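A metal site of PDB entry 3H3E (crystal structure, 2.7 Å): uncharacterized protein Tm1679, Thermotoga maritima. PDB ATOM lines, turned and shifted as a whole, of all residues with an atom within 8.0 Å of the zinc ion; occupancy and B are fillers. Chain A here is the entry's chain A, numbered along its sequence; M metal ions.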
ATOM      1  N   HIS A  31     -24.140   1.627  -2.384  1.00  0.00           N
ATOM      2  CA  HIS A  31     -22.704   1.572  -2.602  1.00  0.00           C
ATOM      3  C   HIS A  31     -22.387   2.294  -3.907  1.00  0.00           C
ATOM      4  O   HIS A  31     -22.494   1.718  -4.990  1.00  0.00           O
ATOM      5  CB  HIS A  31     -22.243   0.131  -2.688  1.00  0.00           C
ATOM      6  CG  HIS A  31     -20.770  -0.023  -2.817  1.00  0.00           C
ATOM      7  ND1 HIS A  31     -19.879   0.517  -1.910  1.00  0.00           N
ATOM      8  CD2 HIS A  31     -20.019  -0.677  -3.741  1.00  0.00           C
ATOM      9  CE1 HIS A  31     -18.652   0.204  -2.273  1.00  0.00           C
ATOM     10  NE2 HIS A  31     -18.709  -0.523  -3.380  1.00  0.00           N
ATOM     11  N   ASP A  43     -19.234  12.303 -10.456  1.00  0.00           N
ATOM     12  CA  ASP A  43     -19.724  10.929 -10.333  1.00  0.00           C
ATOM     13  C   ASP A  43     -21.256  10.827 -10.237  1.00  0.00           C
ATOM     14  O   ASP A  43     -21.959  11.809 -10.034  1.00  0.00           O
ATOM     15  CB  ASP A  43     -19.013  10.182  -9.190  1.00  0.00           C
ATOM     16  CG  ASP A  43     -17.592   9.798  -9.557  1.00  0.00           C
ATOM     17  OD1 ASP A  43     -17.196  10.045 -10.706  1.00  0.00           O
ATOM     18  OD2 ASP A  43     -16.863   9.247  -8.705  1.00  0.00           O
ATOM     19  N   SER A  68     -14.738  10.174 -12.156  1.00  0.00           N
ATOM     20  CA  SER A  68     -13.459   9.983 -11.485  1.00  0.00           C
ATOM     21  C   SER A  68     -12.726   8.737 -11.989  1.00  0.00           C
ATOM     22  O   SER A  68     -11.511   8.720 -12.058  1.00  0.00           O
ATOM     23  CB  SER A  68     -13.672   9.889  -9.988  1.00  0.00           C
ATOM     24  OG  SER A  68     -14.586   8.864  -9.672  1.00  0.00           O
ATOM     25  N   HIS A  69     -13.478   7.693 -12.306  1.00  0.00           N
ATOM     26  CA  HIS A  69     -12.911   6.493 -12.887  1.00  0.00           C
ATOM     27  C   HIS A  69     -14.050   5.580 -13.381  1.00  0.00           C
ATOM     28  O   HIS A  69     -15.196   5.738 -12.987  1.00  0.00           O
ATOM     29  CB  HIS A  69     -11.947   5.786 -11.924  1.00  0.00           C
ATOM     30  CG  HIS A  69     -12.593   5.258 -10.678  1.00  0.00           C
ATOM     31  ND1 HIS A  69     -13.316   6.057  -9.808  1.00  0.00           N
ATOM     32  CD2 HIS A  69     -12.604   4.012 -10.138  1.00  0.00           C
ATOM     33  CE1 HIS A  69     -13.763   5.322  -8.805  1.00  0.00           C
ATOM     34  NE2 HIS A  69     -13.342   4.078  -8.982  1.00  0.00           N
ATOM     35  N   GLY A  70     -13.732   4.650 -14.273  1.00  0.00           N
ATOM     36  CA  GLY A  70     -14.771   3.835 -14.887  1.00  0.00           C
ATOM     37  C   GLY A  70     -15.256   2.606 -14.139  1.00  0.00           C
ATOM     38  O   GLY A  70     -15.479   1.583 -14.759  1.00  0.00           O
ATOM     39  N   HIS A  71     -15.411   2.698 -12.822  1.00  0.00           N
ATOM     40  CA  HIS A  71     -16.091   1.656 -12.060  1.00  0.00           C
ATOM     41  C   HIS A  71     -17.606   1.841 -12.064  1.00  0.00           C
ATOM     42  O   HIS A  71     -18.115   2.966 -12.140  1.00  0.00           O
ATOM     43  CB  HIS A  71     -15.605   1.642 -10.616  1.00  0.00           C
ATOM     44  CG  HIS A  71     -14.476   0.697 -10.370  1.00  0.00           C
ATOM     45  ND1 HIS A  71     -13.467   0.967  -9.471  1.00  0.00           N
ATOM     46  CD2 HIS A  71     -14.196  -0.515 -10.914  1.00  0.00           C
ATOM     47  CE1 HIS A  71     -12.608  -0.045  -9.467  1.00  0.00           C
ATOM     48  NE2 HIS A  71     -13.026  -0.958 -10.327  1.00  0.00           N
ATOM     49  N   TYR A  72     -18.331   0.730 -11.969  1.00  0.00           N
ATOM     50  CA  TYR A  72     -19.801   0.693 -11.982  1.00  0.00           C
ATOM     51  C   TYR A  72     -20.458   1.608 -10.932  1.00  0.00           C
ATOM     52  O   TYR A  72     -21.481   2.216 -11.206  1.00  0.00           O
ATOM     53  CB  TYR A  72     -20.276  -0.753 -11.781  1.00  0.00           C
ATOM     54  CG  TYR A  72     -20.116  -1.236 -10.361  1.00  0.00           C
ATOM     55  CD1 TYR A  72     -21.202  -1.291  -9.498  1.00  0.00           C
ATOM     56  CD2 TYR A  72     -18.875  -1.590  -9.884  1.00  0.00           C
ATOM     57  CE1 TYR A  72     -21.041  -1.706  -8.191  1.00  0.00           C
ATOM     58  CE2 TYR A  72     -18.704  -2.004  -8.579  1.00  0.00           C
ATOM     59  CZ  TYR A  72     -19.794  -2.060  -7.738  1.00  0.00           C
ATOM     60  OH  TYR A  72     -19.623  -2.487  -6.437  1.00  0.00           O
ATOM     61  N   ASP A  73     -19.892   1.675  -9.731  1.00  0.00           N
ATOM     62  CA  ASP A  73     -20.466   2.453  -8.636  1.00  0.00           C
ATOM     63  C   ASP A  73     -20.206   3.960  -8.779  1.00  0.00           C
ATOM     64  O   ASP A  73     -20.638   4.735  -7.929  1.00  0.00           O
ATOM     65  CB  ASP A  73     -19.976   1.943  -7.251  1.00  0.00           C
ATOM     66  CG  ASP A  73     -18.455   1.908  -7.120  1.00  0.00           C
ATOM     67  OD1 ASP A  73     -17.810   1.385  -8.048  1.00  0.00           O
ATOM     68  OD2 ASP A  73     -17.879   2.389  -6.104  1.00  0.00           O
ATOM     69  N   HIS A  74     -19.538   4.361  -9.853  1.00  0.00           N
ATOM     70  CA  HIS A  74     -19.251   5.780 -10.092  1.00  0.00           C
ATOM     71  C   HIS A  74     -19.830   6.246 -11.408  1.00  0.00           C
ATOM     72  O   HIS A  74     -20.268   7.382 -11.546  1.00  0.00           O
ATOM     73  CB  HIS A  74     -17.747   6.063 -10.015  1.00  0.00           C
ATOM     74  CG  HIS A  74     -17.169   5.749  -8.683  1.00  0.00           C
ATOM     75  ND1 HIS A  74     -16.807   6.723  -7.778  1.00  0.00           N
ATOM     76  CD2 HIS A  74     -16.975   4.556  -8.053  1.00  0.00           C
ATOM     77  CE1 HIS A  74     -16.370   6.143  -6.666  1.00  0.00           C
ATOM     78  NE2 HIS A  74     -16.467   4.832  -6.801  1.00  0.00           N
ATOM     79  N   LYS A  96     -13.274  -2.969 -16.690  1.00  0.00           N
ATOM     80  CA  LYS A  96     -12.656  -3.174 -15.396  1.00  0.00           C
ATOM     81  C   LYS A  96     -13.178  -4.408 -14.696  1.00  0.00           C
ATOM     82  O   LYS A  96     -14.377  -4.667 -14.696  1.00  0.00           O
ATOM     83  CB  LYS A  96     -12.880  -1.956 -14.503  1.00  0.00           C
ATOM     84  CG  LYS A  96     -12.108  -0.723 -14.912  1.00  0.00           C
ATOM     85  CD  LYS A  96     -12.024   0.244 -13.727  1.00  0.00           C
ATOM     86  CE  LYS A  96     -11.435   1.588 -14.119  1.00  0.00           C
ATOM     87  NZ  LYS A  96     -10.012   1.472 -14.485  1.00  0.00           N
ATOM     88  N   ALA A 103     -16.600  -5.180 -13.169  1.00  0.00           N
ATOM     89  CA  ALA A 103     -16.893  -3.943 -12.455  1.00  0.00           C
ATOM     90  C   ALA A 103     -16.847  -2.706 -13.345  1.00  0.00           C
ATOM     91  O   ALA A 103     -16.688  -1.598 -12.859  1.00  0.00           O
ATOM     92  CB  ALA A 103     -15.931  -3.776 -11.295  1.00  0.00           C
ATOM     93  N   PHE A 147      -7.624  -5.653  -8.470  1.00  0.00           N
ATOM     94  CA  PHE A 147      -8.186  -5.031  -9.652  1.00  0.00           C
ATOM     95  C   PHE A 147      -7.494  -5.432 -10.963  1.00  0.00           C
ATOM     96  O   PHE A 147      -6.270  -5.489 -11.047  1.00  0.00           O
ATOM     97  CB  PHE A 147      -8.201  -3.517  -9.489  1.00  0.00           C
ATOM     98  CG  PHE A 147      -9.040  -3.069  -8.326  1.00  0.00           C
ATOM     99  CD1 PHE A 147     -10.418  -3.215  -8.355  1.00  0.00           C
ATOM    100  CD2 PHE A 147      -8.451  -2.485  -7.216  1.00  0.00           C
ATOM    101  CE1 PHE A 147     -11.190  -2.818  -7.290  1.00  0.00           C
ATOM    102  CE2 PHE A 147      -9.221  -2.093  -6.138  1.00  0.00           C
ATOM    103  CZ  PHE A 147     -10.591  -2.257  -6.181  1.00  0.00           C
ATOM    104  N   ASP A 158      -4.787  -3.594 -13.037  1.00  0.00           N
ATOM    105  CA  ASP A 158      -5.337  -2.245 -13.264  1.00  0.00           C
ATOM    106  C   ASP A 158      -4.622  -1.208 -12.420  1.00  0.00           C
ATOM    107  O   ASP A 158      -4.654  -1.286 -11.183  1.00  0.00           O
ATOM    108  CB  ASP A 158      -6.844  -2.242 -12.931  1.00  0.00           C
ATOM    109  CG  ASP A 158      -7.556  -0.984 -13.427  1.00  0.00           C
ATOM    110  OD1 ASP A 158      -6.902  -0.088 -14.001  1.00  0.00           O
ATOM    111  OD2 ASP A 158      -8.782  -0.892 -13.225  1.00  0.00           O
ATOM    112  N   PHE A 160      -5.269   2.093 -12.924  1.00  0.00           N
ATOM    113  CA  PHE A 160      -6.205   3.205 -12.887  1.00  0.00           C
ATOM    114  C   PHE A 160      -5.686   4.426 -13.613  1.00  0.00           C
ATOM    115  O   PHE A 160      -5.758   5.550 -13.113  1.00  0.00           O
ATOM    116  CB  PHE A 160      -6.641   3.490 -11.456  1.00  0.00           C
ATOM    117  CG  PHE A 160      -7.415   2.376 -10.846  1.00  0.00           C
ATOM    118  CD1 PHE A 160      -6.769   1.329 -10.220  1.00  0.00           C
ATOM    119  CD2 PHE A 160      -8.789   2.324 -10.956  1.00  0.00           C
ATOM    120  CE1 PHE A 160      -7.484   0.266  -9.678  1.00  0.00           C
ATOM    121  CE2 PHE A 160      -9.513   1.275 -10.408  1.00  0.00           C
ATOM    122  CZ  PHE A 160      -8.865   0.246  -9.769  1.00  0.00           C
ATOM    123  N   ASP A 162      -7.147   5.737 -15.669  1.00  0.00           N
ATOM    124  CA  ASP A 162      -8.376   6.492 -15.941  1.00  0.00           C
ATOM    125  C   ASP A 162      -8.789   7.435 -14.816  1.00  0.00           C
ATOM    126  O   ASP A 162      -9.680   8.238 -14.993  1.00  0.00           O
ATOM    127  CB  ASP A 162      -9.527   5.545 -16.202  1.00  0.00           C
ATOM    128  CG  ASP A 162      -9.754   4.550 -15.068  1.00  0.00           C
ATOM    129  OD1 ASP A 162      -8.759   3.957 -14.594  1.00  0.00           O
ATOM    130  OD2 ASP A 162     -10.918   4.359 -14.656  1.00  0.00           O
ATOM    131  N   GLU A 163      -8.135   7.330 -13.667  1.00  0.00           N
ATOM    132  CA  GLU A 163      -8.530   8.076 -12.470  1.00  0.00           C
ATOM    133  C   GLU A 163      -8.221   9.556 -12.563  1.00  0.00           C
ATOM    134  O   GLU A 163      -7.124   9.942 -12.926  1.00  0.00           O
ATOM    135  CB  GLU A 163      -7.839   7.506 -11.231  1.00  0.00           C
ATOM    136  CG  GLU A 163      -8.241   8.187  -9.956  1.00  0.00           C
ATOM    137  CD  GLU A 163      -7.870   7.363  -8.736  1.00  0.00           C
ATOM    138  OE1 GLU A 163      -6.723   7.476  -8.263  1.00  0.00           O
ATOM    139  OE2 GLU A 163      -8.745   6.610  -8.257  1.00  0.00           O
ATOM    140  N   GLY A 179     -13.158  10.396  -6.072  1.00  0.00           N
ATOM    141  CA  GLY A 179     -14.144   9.329  -6.084  1.00  0.00           C
ATOM    142  C   GLY A 179     -13.699   8.189  -5.214  1.00  0.00           C
ATOM    143  O   GLY A 179     -14.342   7.875  -4.220  1.00  0.00           O
ATOM    144  N   CYS A 180     -12.583   7.559  -5.561  1.00  0.00           N
ATOM    145  CA  CYS A 180     -12.134   6.416  -4.791  1.00  0.00           C
ATOM    146  C   CYS A 180     -10.636   6.463  -4.416  1.00  0.00           C
ATOM    147  O   CYS A 180     -10.198   5.774  -3.509  1.00  0.00           O
ATOM    148  CB  CYS A 180     -12.490   5.114  -5.523  1.00  0.00           C
ATOM    149  SG  CYS A 180     -13.614   4.055  -4.630  1.00  0.00           S
ATOM    150  N   SER A 181      -9.871   7.269  -5.130  1.00  0.00           N
ATOM    151  CA  SER A 181      -8.442   7.410  -4.848  1.00  0.00           C
ATOM    152  C   SER A 181      -7.689   6.092  -4.925  1.00  0.00           C
ATOM    153  O   SER A 181      -7.058   5.694  -3.965  1.00  0.00           O
ATOM    154  CB  SER A 181      -8.218   8.025  -3.475  1.00  0.00           C
ATOM    155  OG  SER A 181      -8.928   9.240  -3.342  1.00  0.00           O
ATOM    156  N   HIS A 182      -7.741   5.420  -6.059  1.00  0.00           N
ATOM    157  CA  HIS A 182      -7.081   4.127  -6.202  1.00  0.00           C
ATOM    158  C   HIS A 182      -5.568   4.278  -6.286  1.00  0.00           C
ATOM    159  O   HIS A 182      -4.814   3.394  -5.903  1.00  0.00           O
ATOM    160  CB  HIS A 182      -7.603   3.404  -7.433  1.00  0.00           C
ATOM    161  CG  HIS A 182      -8.944   2.764  -7.245  1.00  0.00           C
ATOM    162  ND1 HIS A 182      -9.127   1.653  -6.431  1.00  0.00           N
ATOM    163  CD2 HIS A 182     -10.167   3.065  -7.743  1.00  0.00           C
ATOM    164  CE1 HIS A 182     -10.400   1.304  -6.465  1.00  0.00           C
ATOM    165  NE2 HIS A 182     -11.054   2.142  -7.245  1.00  0.00           N
ATOM    166  N   HIS A 208     -10.532   4.796  -0.206  1.00  0.00           N
ATOM    167  CA  HIS A 208     -10.262   3.369  -0.405  1.00  0.00           C
ATOM    168  C   HIS A 208      -9.249   2.819   0.573  1.00  0.00           C
ATOM    169  O   HIS A 208      -8.204   2.291   0.175  1.00  0.00           O
ATOM    170  CB  HIS A 208      -9.826   3.071  -1.841  1.00  0.00           C
ATOM    171  CG  HIS A 208     -10.120   1.677  -2.267  1.00  0.00           C
ATOM    172  ND1 HIS A 208     -11.397   1.241  -2.595  1.00  0.00           N
ATOM    173  CD2 HIS A 208      -9.313   0.589  -2.410  1.00  0.00           C
ATOM    174  CE1 HIS A 208     -11.354  -0.038  -2.924  1.00  0.00           C
ATOM    175  NE2 HIS A 208     -10.109  -0.455  -2.811  1.00  0.00           N
ATOM    176  N   HIS A 236     -17.821   6.936   1.080  1.00  0.00           N
ATOM    177  CA  HIS A 236     -17.759   5.812   0.141  1.00  0.00           C
ATOM    178  C   HIS A 236     -16.759   4.741   0.570  1.00  0.00           C
ATOM    179  O   HIS A 236     -16.870   4.179   1.675  1.00  0.00           O
ATOM    180  CB  HIS A 236     -17.422   6.365  -1.263  1.00  0.00           C
ATOM    181  CG  HIS A 236     -17.584   5.368  -2.377  1.00  0.00           C
ATOM    182  ND1 HIS A 236     -18.621   4.456  -2.426  1.00  0.00           N
ATOM    183  CD2 HIS A 236     -16.858   5.172  -3.501  1.00  0.00           C
ATOM    184  CE1 HIS A 236     -18.503   3.721  -3.520  1.00  0.00           C
ATOM    185  NE2 HIS A 236     -17.437   4.132  -4.195  1.00  0.00           N
ATOM    186  N   CYS A 237     -15.762   4.463  -0.272  1.00  0.00           N
ATOM    187  CA  CYS A 237     -14.783   3.406   0.028  1.00  0.00           C
ATOM    188  C   CYS A 237     -14.007   3.530   1.349  1.00  0.00           C
ATOM    189  O   CYS A 237     -13.583   2.523   1.921  1.00  0.00           O
ATOM    190  CB  CYS A 237     -13.812   3.114  -1.163  1.00  0.00           C
ATOM    191  SG  CYS A 237     -13.615   4.281  -2.581  1.00  0.00           S
HETATM  192 ZN    ZN M   1     -13.383   2.200  -7.663  1.00  0.00          ZN
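A ring nitrogen (ND1) of His 69 is in hydrogen-bond range of the side-chain hydroxyl (OG) of Ser 68.
The backbone NH (N) of His 182 lies within hydrogen-bond range of the side-chain carboxylate (OE2) of Glu 163, 2.7 Å away.
The side-chain sulfur (SG) of Cys 180 lies within hydrogen-bond range of a ring nitrogen (NE2) of His 74 (3.7 Å).
The side-chain sulfur (SG) of Cys 180 forms a disulfide with the side-chain sulfur (SG) of Cys 237 (2.1 Å).
The backbone NH of His 208 sits close to the backbone carbonyl oxygen of Cys 180 (3.5 Å).
Merely in contact with the zinc ion: Cys 180 (3.6 Å).
Four residues have an atom within 4 Å of the zinc ion: His 69, His 71, Cys 180 and His 182.
The nearest printed residue that does not touch the zinc ion is His 74 (4.1 Å).
ND1 of His 71 is bound to the zinc ion.
The zinc ion is bound by a ring nitrogen (NE2) of His 69 (2.3 Å).
The zinc ion is bound by NE2 of His 182 (2.4 Å).
The zinc ion has three donor atoms within binding distance.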
